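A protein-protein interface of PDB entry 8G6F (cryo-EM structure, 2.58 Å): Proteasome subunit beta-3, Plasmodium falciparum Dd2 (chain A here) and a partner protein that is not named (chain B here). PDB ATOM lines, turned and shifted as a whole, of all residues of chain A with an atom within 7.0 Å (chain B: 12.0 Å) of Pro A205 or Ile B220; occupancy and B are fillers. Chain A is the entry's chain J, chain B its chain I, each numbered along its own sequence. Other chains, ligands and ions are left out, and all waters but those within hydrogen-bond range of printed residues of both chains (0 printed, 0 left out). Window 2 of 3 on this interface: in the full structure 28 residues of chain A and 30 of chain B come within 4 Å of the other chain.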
ATOM      1  N   SER A  18       4.383 -11.066 -19.534  1.00  0.00           N
ATOM      2  CA  SER A  18       4.319 -11.579 -20.898  1.00  0.00           C
ATOM      3  C   SER A  18       2.919 -11.312 -21.429  1.00  0.00           C
ATOM      4  O   SER A  18       1.966 -12.015 -21.089  1.00  0.00           O
ATOM      5  CB  SER A  18       4.661 -13.062 -20.936  1.00  0.00           C
ATOM      6  OG  SER A  18       5.200 -13.420 -22.196  1.00  0.00           O
ATOM      7  N   ASN A  19       2.791 -10.285 -22.267  1.00  0.00           N
ATOM      8  CA  ASN A  19       1.515  -9.907 -22.860  1.00  0.00           C
ATOM      9  C   ASN A  19       0.533  -9.387 -21.814  1.00  0.00           C
ATOM     10  O   ASN A  19      -0.677  -9.574 -21.936  1.00  0.00           O
ATOM     11  CB  ASN A  19       0.901 -11.079 -23.631  1.00  0.00           C
ATOM     12  CG  ASN A  19       0.431 -10.682 -25.010  1.00  0.00           C
ATOM     13  OD1 ASN A  19       1.168 -10.061 -25.773  1.00  0.00           O
ATOM     14  ND2 ASN A  19      -0.801 -11.044 -25.342  1.00  0.00           N
ATOM     15  N   CYS A  20       1.049  -8.730 -20.782  1.00  0.00           N
ATOM     16  CA  CYS A  20       0.214  -8.129 -19.755  1.00  0.00           C
ATOM     17  C   CYS A  20       1.039  -7.090 -19.019  1.00  0.00           C
ATOM     18  O   CYS A  20       2.269  -7.139 -19.018  1.00  0.00           O
ATOM     19  CB  CYS A  20      -0.328  -9.181 -18.782  1.00  0.00           C
ATOM     20  SG  CYS A  20       0.922 -10.269 -18.088  1.00  0.00           S
ATOM     21  N   VAL A  21       0.345  -6.142 -18.394  1.00  0.00           N
ATOM     22  CA  VAL A  21       0.973  -5.181 -17.499  1.00  0.00           C
ATOM     23  C   VAL A  21       0.168  -5.146 -16.211  1.00  0.00           C
ATOM     24  O   VAL A  21      -0.890  -5.755 -16.099  1.00  0.00           O
ATOM     25  CB  VAL A  21       1.095  -3.760 -18.103  1.00  0.00           C
ATOM     26  CG1 VAL A  21       2.308  -3.667 -18.982  1.00  0.00           C
ATOM     27  CG2 VAL A  21      -0.142  -3.364 -18.881  1.00  0.00           C
ATOM     28  N   LYS A  46      -7.831   5.706 -15.638  1.00  0.00           N
ATOM     29  CA  LYS A  46      -7.854   5.142 -16.979  1.00  0.00           C
ATOM     30  C   LYS A  46      -8.007   6.269 -17.991  1.00  0.00           C
ATOM     31  O   LYS A  46      -8.962   7.047 -17.915  1.00  0.00           O
ATOM     32  CB  LYS A  46      -8.995   4.137 -17.111  1.00  0.00           C
ATOM     33  CG  LYS A  46      -9.089   3.470 -18.464  1.00  0.00           C
ATOM     34  CD  LYS A  46     -10.446   2.838 -18.672  1.00  0.00           C
ATOM     35  CE  LYS A  46     -10.628   2.398 -20.106  1.00  0.00           C
ATOM     36  NZ  LYS A  46     -11.878   1.626 -20.300  1.00  0.00           N
ATOM     37  N   ASN A  49      -8.506   2.414 -23.170  1.00  0.00           N
ATOM     38  CA  ASN A  49      -8.394   0.984 -22.908  1.00  0.00           C
ATOM     39  C   ASN A  49      -6.952   0.545 -22.708  1.00  0.00           C
ATOM     40  O   ASN A  49      -6.695  -0.400 -21.956  1.00  0.00           O
ATOM     41  CB  ASN A  49      -9.023   0.192 -24.053  1.00  0.00           C
ATOM     42  CG  ASN A  49     -10.485  -0.093 -23.825  1.00  0.00           C
ATOM     43  OD1 ASN A  49     -10.919  -0.311 -22.698  1.00  0.00           O
ATOM     44  ND2 ASN A  49     -11.257  -0.099 -24.900  1.00  0.00           N
ATOM     45  N   ASN A  50      -6.001   1.203 -23.366  1.00  0.00           N
ATOM     46  CA  ASN A  50      -4.609   0.773 -23.354  1.00  0.00           C
ATOM     47  C   ASN A  50      -3.691   1.726 -22.606  1.00  0.00           C
ATOM     48  O   ASN A  50      -2.473   1.561 -22.676  1.00  0.00           O
ATOM     49  CB  ASN A  50      -4.100   0.604 -24.786  1.00  0.00           C
ATOM     50  CG  ASN A  50      -4.978  -0.294 -25.609  1.00  0.00           C
ATOM     51  OD1 ASN A  50      -5.494   0.111 -26.647  1.00  0.00           O
ATOM     52  ND2 ASN A  50      -5.156  -1.524 -25.154  1.00  0.00           N
ATOM     53  N   TYR A  52      -3.141   3.789 -18.810  1.00  0.00           N
ATOM     54  CA  TYR A  52      -3.463   4.123 -17.438  1.00  0.00           C
ATOM     55  C   TYR A  52      -2.357   5.009 -16.898  1.00  0.00           C
ATOM     56  O   TYR A  52      -1.195   4.889 -17.295  1.00  0.00           O
ATOM     57  CB  TYR A  52      -3.597   2.877 -16.559  1.00  0.00           C
ATOM     58  CG  TYR A  52      -4.864   2.100 -16.790  1.00  0.00           C
ATOM     59  CD1 TYR A  52      -5.052   1.374 -17.952  1.00  0.00           C
ATOM     60  CD2 TYR A  52      -5.875   2.095 -15.848  1.00  0.00           C
ATOM     61  CE1 TYR A  52      -6.207   0.668 -18.167  1.00  0.00           C
ATOM     62  CE2 TYR A  52      -7.028   1.392 -16.056  1.00  0.00           C
ATOM     63  CZ  TYR A  52      -7.190   0.678 -17.215  1.00  0.00           C
ATOM     64  OH  TYR A  52      -8.346  -0.027 -17.425  1.00  0.00           O
ATOM     65  N   PHE A 114      -0.312  -0.341 -23.094  1.00  0.00           N
ATOM     66  CA  PHE A 114       0.017  -1.194 -24.226  1.00  0.00           C
ATOM     67  C   PHE A 114       0.306  -0.337 -25.445  1.00  0.00           C
ATOM     68  O   PHE A 114      -0.460   0.577 -25.762  1.00  0.00           O
ATOM     69  CB  PHE A 114      -1.126  -2.156 -24.546  1.00  0.00           C
ATOM     70  CG  PHE A 114      -1.171  -3.360 -23.665  1.00  0.00           C
ATOM     71  CD1 PHE A 114      -0.087  -4.210 -23.574  1.00  0.00           C
ATOM     72  CD2 PHE A 114      -2.302  -3.649 -22.934  1.00  0.00           C
ATOM     73  CE1 PHE A 114      -0.131  -5.319 -22.769  1.00  0.00           C
ATOM     74  CE2 PHE A 114      -2.347  -4.758 -22.127  1.00  0.00           C
ATOM     75  CZ  PHE A 114      -1.262  -5.592 -22.046  1.00  0.00           C
ATOM     76  N   VAL A 128      -2.926  -7.788 -34.288  1.00  0.00           N
ATOM     77  CA  VAL A 128      -2.246  -6.658 -33.667  1.00  0.00           C
ATOM     78  C   VAL A 128      -1.425  -7.177 -32.497  1.00  0.00           C
ATOM     79  O   VAL A 128      -1.859  -8.079 -31.772  1.00  0.00           O
ATOM     80  CB  VAL A 128      -3.246  -5.583 -33.197  1.00  0.00           C
ATOM     81  CG1 VAL A 128      -4.400  -6.225 -32.450  1.00  0.00           C
ATOM     82  CG2 VAL A 128      -2.552  -4.552 -32.324  1.00  0.00           C
ATOM     83  N   ASN A 129      -0.236  -6.612 -32.319  1.00  0.00           N
ATOM     84  CA  ASN A 129       0.675  -7.006 -31.254  1.00  0.00           C
ATOM     85  C   ASN A 129       0.626  -5.973 -30.136  1.00  0.00           C
ATOM     86  O   ASN A 129       0.730  -4.769 -30.391  1.00  0.00           O
ATOM     87  CB  ASN A 129       2.101  -7.142 -31.786  1.00  0.00           C
ATOM     88  CG  ASN A 129       3.020  -7.837 -30.807  1.00  0.00           C
ATOM     89  OD1 ASN A 129       2.963  -9.055 -30.647  1.00  0.00           O
ATOM     90  ND2 ASN A 129       3.875  -7.068 -30.148  1.00  0.00           N
ATOM     91  N   TYR A 130       0.467  -6.450 -28.906  1.00  0.00           N
ATOM     92  CA  TYR A 130       0.403  -5.600 -27.725  1.00  0.00           C
ATOM     93  C   TYR A 130       1.741  -5.680 -27.006  1.00  0.00           C
ATOM     94  O   TYR A 130       2.133  -6.751 -26.534  1.00  0.00           O
ATOM     95  CB  TYR A 130      -0.729  -6.036 -26.801  1.00  0.00           C
ATOM     96  CG  TYR A 130      -2.108  -5.718 -27.318  1.00  0.00           C
ATOM     97  CD1 TYR A 130      -2.598  -6.328 -28.459  1.00  0.00           C
ATOM     98  CD2 TYR A 130      -2.925  -4.821 -26.656  1.00  0.00           C
ATOM     99  CE1 TYR A 130      -3.854  -6.045 -28.931  1.00  0.00           C
ATOM    100  CE2 TYR A 130      -4.183  -4.534 -27.120  1.00  0.00           C
ATOM    101  CZ  TYR A 130      -4.644  -5.150 -28.258  1.00  0.00           C
ATOM    102  OH  TYR A 130      -5.902  -4.863 -28.728  1.00  0.00           O
ATOM    103  N   LEU A 203      -3.670  -5.559 -16.597  1.00  0.00           N
ATOM    104  CA  LEU A 203      -4.116  -5.349 -17.962  1.00  0.00           C
ATOM    105  C   LEU A 203      -3.670  -6.508 -18.836  1.00  0.00           C
ATOM    106  O   LEU A 203      -2.486  -6.866 -18.855  1.00  0.00           O
ATOM    107  CB  LEU A 203      -3.552  -4.049 -18.527  1.00  0.00           C
ATOM    108  CG  LEU A 203      -4.356  -2.768 -18.362  1.00  0.00           C
ATOM    109  CD1 LEU A 203      -4.134  -2.178 -16.985  1.00  0.00           C
ATOM    110  CD2 LEU A 203      -3.948  -1.789 -19.451  1.00  0.00           C
ATOM    111  N   THR A 204      -4.622  -7.072 -19.560  1.00  0.00           N
ATOM    112  CA  THR A 204      -4.438  -8.067 -20.594  1.00  0.00           C
ATOM    113  C   THR A 204      -5.111  -7.528 -21.846  1.00  0.00           C
ATOM    114  O   THR A 204      -6.037  -6.720 -21.741  1.00  0.00           O
ATOM    115  CB  THR A 204      -5.064  -9.404 -20.169  1.00  0.00           C
ATOM    116  OG1 THR A 204      -4.389  -9.896 -19.007  1.00  0.00           O
ATOM    117  CG2 THR A 204      -4.969 -10.442 -21.252  1.00  0.00           C
ATOM    118  N   PRO A 205      -4.661  -7.918 -23.039  1.00  0.00           N
ATOM    119  CA  PRO A 205      -5.269  -7.334 -24.242  1.00  0.00           C
ATOM    120  C   PRO A 205      -6.774  -7.530 -24.325  1.00  0.00           C
ATOM    121  O   PRO A 205      -7.449  -6.736 -24.991  1.00  0.00           O
ATOM    122  CB  PRO A 205      -4.533  -8.050 -25.379  1.00  0.00           C
ATOM    123  CG  PRO A 205      -3.213  -8.345 -24.813  1.00  0.00           C
ATOM    124  CD  PRO A 205      -3.456  -8.694 -23.379  1.00  0.00           C
ATOM    125  N   GLU A 206      -7.328  -8.550 -23.667  1.00  0.00           N
ATOM    126  CA  GLU A 206      -8.752  -8.835 -23.761  1.00  0.00           C
ATOM    127  C   GLU A 206      -9.551  -8.489 -22.515  1.00  0.00           C
ATOM    128  O   GLU A 206     -10.776  -8.394 -22.607  1.00  0.00           O
ATOM    129  CB  GLU A 206      -8.979 -10.320 -24.083  1.00  0.00           C
ATOM    130  CG  GLU A 206      -8.423 -11.283 -23.048  1.00  0.00           C
ATOM    131  CD  GLU A 206      -7.031 -11.773 -23.386  1.00  0.00           C
ATOM    132  OE1 GLU A 206      -6.478 -11.345 -24.421  1.00  0.00           O
ATOM    133  OE2 GLU A 206      -6.487 -12.587 -22.613  1.00  0.00           O
ATOM    134  N   LYS A 207      -8.912  -8.304 -21.363  1.00  0.00           N
ATOM    135  CA  LYS A 207      -9.663  -8.017 -20.149  1.00  0.00           C
ATOM    136  C   LYS A 207      -8.768  -7.316 -19.140  1.00  0.00           C
ATOM    137  O   LYS A 207      -7.541  -7.346 -19.238  1.00  0.00           O
ATOM    138  CB  LYS A 207     -10.255  -9.295 -19.547  1.00  0.00           C
ATOM    139  CG  LYS A 207      -9.259 -10.182 -18.833  1.00  0.00           C
ATOM    140  CD  LYS A 207      -9.911 -11.492 -18.431  1.00  0.00           C
ATOM    141  CE  LYS A 207      -8.933 -12.463 -17.788  1.00  0.00           C
ATOM    142  NZ  LYS A 207      -7.528 -12.265 -18.222  1.00  0.00           N
ATOM    143  N   ILE A 208      -9.416  -6.681 -18.167  1.00  0.00           N
ATOM    144  CA  ILE A 208      -8.758  -6.013 -17.052  1.00  0.00           C
ATOM    145  C   ILE A 208      -9.279  -6.637 -15.766  1.00  0.00           C
ATOM    146  O   ILE A 208     -10.493  -6.773 -15.585  1.00  0.00           O
ATOM    147  CB  ILE A 208      -9.009  -4.492 -17.074  1.00  0.00           C
ATOM    148  CG1 ILE A 208      -8.300  -3.795 -15.911  1.00  0.00           C
ATOM    149  CG2 ILE A 208     -10.485  -4.189 -17.019  1.00  0.00           C
ATOM    150  CD1 ILE A 208      -6.921  -3.317 -16.241  1.00  0.00           C
ATOM    151  N   ILE A 209      -8.365  -7.020 -14.882  1.00  0.00           N
ATOM    152  CA  ILE A 209      -8.702  -7.604 -13.590  1.00  0.00           C
ATOM    153  C   ILE A 209      -8.368  -6.578 -12.517  1.00  0.00           C
ATOM    154  O   ILE A 209      -7.215  -6.151 -12.397  1.00  0.00           O
ATOM    155  CB  ILE A 209      -7.948  -8.921 -13.347  1.00  0.00           C
ATOM    156  CG1 ILE A 209      -8.278  -9.940 -14.437  1.00  0.00           C
ATOM    157  CG2 ILE A 209      -8.294  -9.493 -11.987  1.00  0.00           C
ATOM    158  CD1 ILE A 209      -7.067 -10.634 -14.991  1.00  0.00           C
ATOM    159  N   LYS A 210      -9.372  -6.186 -11.740  1.00  0.00           N
ATOM    160  CA  LYS A 210      -9.211  -5.235 -10.648  1.00  0.00           C
ATOM    161  C   LYS A 210      -9.352  -5.970  -9.326  1.00  0.00           C
ATOM    162  O   LYS A 210     -10.352  -6.655  -9.098  1.00  0.00           O
ATOM    163  CB  LYS A 210     -10.250  -4.119 -10.728  1.00  0.00           C
ATOM    164  CG  LYS A 210     -10.002  -3.114 -11.823  1.00  0.00           C
ATOM    165  CD  LYS A 210     -11.263  -2.340 -12.160  1.00  0.00           C
ATOM    166  CE  LYS A 210     -11.675  -2.568 -13.598  1.00  0.00           C
ATOM    167  NZ  LYS A 210     -12.039  -3.989 -13.850  1.00  0.00           N
ATOM    168  N   LYS B 216     -12.913  -7.769  -9.241  1.00  0.00           N
ATOM    169  CA  LYS B 216     -13.830  -7.416 -10.312  1.00  0.00           C
ATOM    170  C   LYS B 216     -13.109  -7.601 -11.637  1.00  0.00           C
ATOM    171  O   LYS B 216     -12.014  -7.066 -11.826  1.00  0.00           O
ATOM    172  CB  LYS B 216     -14.314  -5.969 -10.177  1.00  0.00           C
ATOM    173  CG  LYS B 216     -15.175  -5.672  -8.943  1.00  0.00           C
ATOM    174  CD  LYS B 216     -14.386  -5.606  -7.625  1.00  0.00           C
ATOM    175  CE  LYS B 216     -13.333  -4.495  -7.593  1.00  0.00           C
ATOM    176  NZ  LYS B 216     -12.185  -4.838  -6.709  1.00  0.00           N
ATOM    177  N   ILE B 217     -13.713  -8.357 -12.547  1.00  0.00           N
ATOM    178  CA  ILE B 217     -13.145  -8.613 -13.864  1.00  0.00           C
ATOM    179  C   ILE B 217     -14.021  -7.935 -14.905  1.00  0.00           C
ATOM    180  O   ILE B 217     -15.243  -8.126 -14.919  1.00  0.00           O
ATOM    181  CB  ILE B 217     -13.019 -10.117 -14.152  1.00  0.00           C
ATOM    182  CG1 ILE B 217     -12.167 -10.786 -13.074  1.00  0.00           C
ATOM    183  CG2 ILE B 217     -12.412 -10.342 -15.533  1.00  0.00           C
ATOM    184  CD1 ILE B 217     -12.036 -12.278 -13.239  1.00  0.00           C
ATOM    185  N   GLU B 218     -13.396  -7.147 -15.770  1.00  0.00           N
ATOM    186  CA  GLU B 218     -14.070  -6.473 -16.866  1.00  0.00           C
ATOM    187  C   GLU B 218     -13.404  -6.874 -18.171  1.00  0.00           C
ATOM    188  O   GLU B 218     -12.190  -7.089 -18.216  1.00  0.00           O
ATOM    189  CB  GLU B 218     -14.022  -4.958 -16.692  1.00  0.00           C
ATOM    190  CG  GLU B 218     -15.038  -4.209 -17.531  1.00  0.00           C
ATOM    191  CD  GLU B 218     -14.459  -2.966 -18.173  1.00  0.00           C
ATOM    192  OE1 GLU B 218     -13.555  -2.349 -17.570  1.00  0.00           O
ATOM    193  OE2 GLU B 218     -14.907  -2.606 -19.281  1.00  0.00           O
ATOM    194  N   TYR B 219     -14.198  -6.980 -19.229  1.00  0.00           N
ATOM    195  CA  TYR B 219     -13.707  -7.405 -20.531  1.00  0.00           C
ATOM    196  C   TYR B 219     -13.565  -6.198 -21.443  1.00  0.00           C
ATOM    197  O   TYR B 219     -14.491  -5.391 -21.566  1.00  0.00           O
ATOM    198  CB  TYR B 219     -14.642  -8.438 -21.154  1.00  0.00           C
ATOM    199  CG  TYR B 219     -14.462  -9.810 -20.562  1.00  0.00           C
ATOM    200  CD1 TYR B 219     -13.396 -10.610 -20.941  1.00  0.00           C
ATOM    201  CD2 TYR B 219     -15.345 -10.301 -19.613  1.00  0.00           C
ATOM    202  CE1 TYR B 219     -13.220 -11.859 -20.400  1.00  0.00           C
ATOM    203  CE2 TYR B 219     -15.175 -11.552 -19.066  1.00  0.00           C
ATOM    204  CZ  TYR B 219     -14.111 -12.327 -19.463  1.00  0.00           C
ATOM    205  OH  TYR B 219     -13.933 -13.577 -18.924  1.00  0.00           O
ATOM    206  N   ILE B 220     -12.405  -6.077 -22.070  1.00  0.00           N
ATOM    207  CA  ILE B 220     -12.112  -4.971 -22.969  1.00  0.00           C
ATOM    208  C   ILE B 220     -12.565  -5.367 -24.365  1.00  0.00           C
ATOM    209  O   ILE B 220     -12.222  -6.447 -24.857  1.00  0.00           O
ATOM    210  CB  ILE B 220     -10.614  -4.623 -22.944  1.00  0.00           C
ATOM    211  CG1 ILE B 220     -10.306  -3.675 -21.786  1.00  0.00           C
ATOM    212  CG2 ILE B 220     -10.181  -3.981 -24.252  1.00  0.00           C
ATOM    213  CD1 ILE B 220     -10.881  -4.111 -20.458  1.00  0.00           C
ATOM    214  N   LYS B 221     -13.345  -4.499 -24.998  1.00  0.00           N
ATOM    215  CA  LYS B 221     -13.920  -4.799 -26.300  1.00  0.00           C
ATOM    216  C   LYS B 221     -13.462  -3.788 -27.345  1.00  0.00           C
ATOM    217  O   LYS B 221     -12.619  -4.093 -28.188  1.00  0.00           O
ATOM    218  CB  LYS B 221     -15.447  -4.814 -26.210  1.00  0.00           C
ATOM    219  CG  LYS B 221     -15.993  -5.742 -25.134  1.00  0.00           C
ATOM    220  CD  LYS B 221     -17.456  -5.457 -24.833  1.00  0.00           C
ATOM    221  CE  LYS B 221     -18.378  -6.244 -25.746  1.00  0.00           C
ATOM    222  NZ  LYS B 221     -18.682  -7.596 -25.204  1.00  0.00           N
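Among the printed residues, pairs that only touch across the chains: Asn A49 with Ile B220 (3.5 Å), Pro A205 with Ile B220 (3.9 Å), Glu A206 with Tyr B219 (3.7 Å), Lys A207 with Ile B217 (3.997 Å), Lys A207 with Glu B218 (3.2 Å), Lys A207 with Tyr B219 (3.7 Å), Lys A207 with Ile B220 (3.9 Å), Ile A208 with Ile B217 (3.7 Å), Ile A208 with Ile B220 (3.5 Å), Ile A209 with Lys B216 (3.7 Å) and Lys A210 with Glu B218 (3.6 Å).
Of chain B, only Ile B220 (3.9 Å) comes within 4 Å of Pro A205. Ile B220 touches just these residues of chain A: Asn A49, Pro A205, Glu A206, Lys A207 and Ile A208. Asn A19 touches none of the printed residues of chain B. No residue of chain B comes within 4 Å of Tyr A130. No residue of chain B comes within 4 Å of Leu A203. No residue of chain B comes within 4 Å of Thr A204. Of chain B, only Tyr B219 (3.7 Å) and Ile B220 (2.9 Å) come within 4 Å of Glu A206. Printed residues of chain B within 4 Å of Ile A208: Ile B217, Glu B218 and Ile B220. Printed residues of chain A within 4 Å of Lys B216: Ile A209 and Lys A210. Of the printed residues of chain A, Tyr B219 touches Glu A206 (3.7 Å) and Lys A207 (3.7 Å). Of the printed residues of chain B, Lys A210 touches Lys B216 (2.8 Å) and Glu B218 (3.6 Å). Phe A114 touches none of the printed residues of chain B. Asn A50 touches none of the printed residues of chain B. The nearest printed residue of chain A that does not touch Glu B218 is Glu A206 (4.8 Å).
Of the 6 printed residues of chain B, 5 touch a printed residue of chain A. Printed residues of chain B that touch a printed residue of chain A: Lys B216, Ile B217, Glu B218, Tyr B219 and Ile B220. Hydrophobic or aromatic side chains of chain B that line the printed part of chain A: Ile B217, Tyr B219 and Ile B220. Of the 20 printed residues of chain A, 7 touch a printed residue of chain B. Printed residues of chain A that touch a printed residue of chain B: Asn A49, Pro A205, Glu A206, Lys A207, Ile A208, Ile A209 and Lys A210. Among the printed residues, no Asp or Glu carboxylate lies within 4 Å of a Lys or Arg side-chain nitrogen of the other chain.
The backbone NH (N) of Ile B220 is in hydrogen-bond range of the backbone carbonyl oxygen (O) of Glu A206 (2.9 Å). The backbone NH (N) of Ile A208 sits at hydrogen-bond distance from the backbone carbonyl oxygen (O) of Glu B218, at 2.8 Å. N of Lys A210 is in hydrogen-bond range of O of Lys B216, 2.8 Å away.
The side-chain amide oxygen (OD1) of Asn A49 lies within hydrogen-bond range of the side-chain amino group (NZ) of Lys A46.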
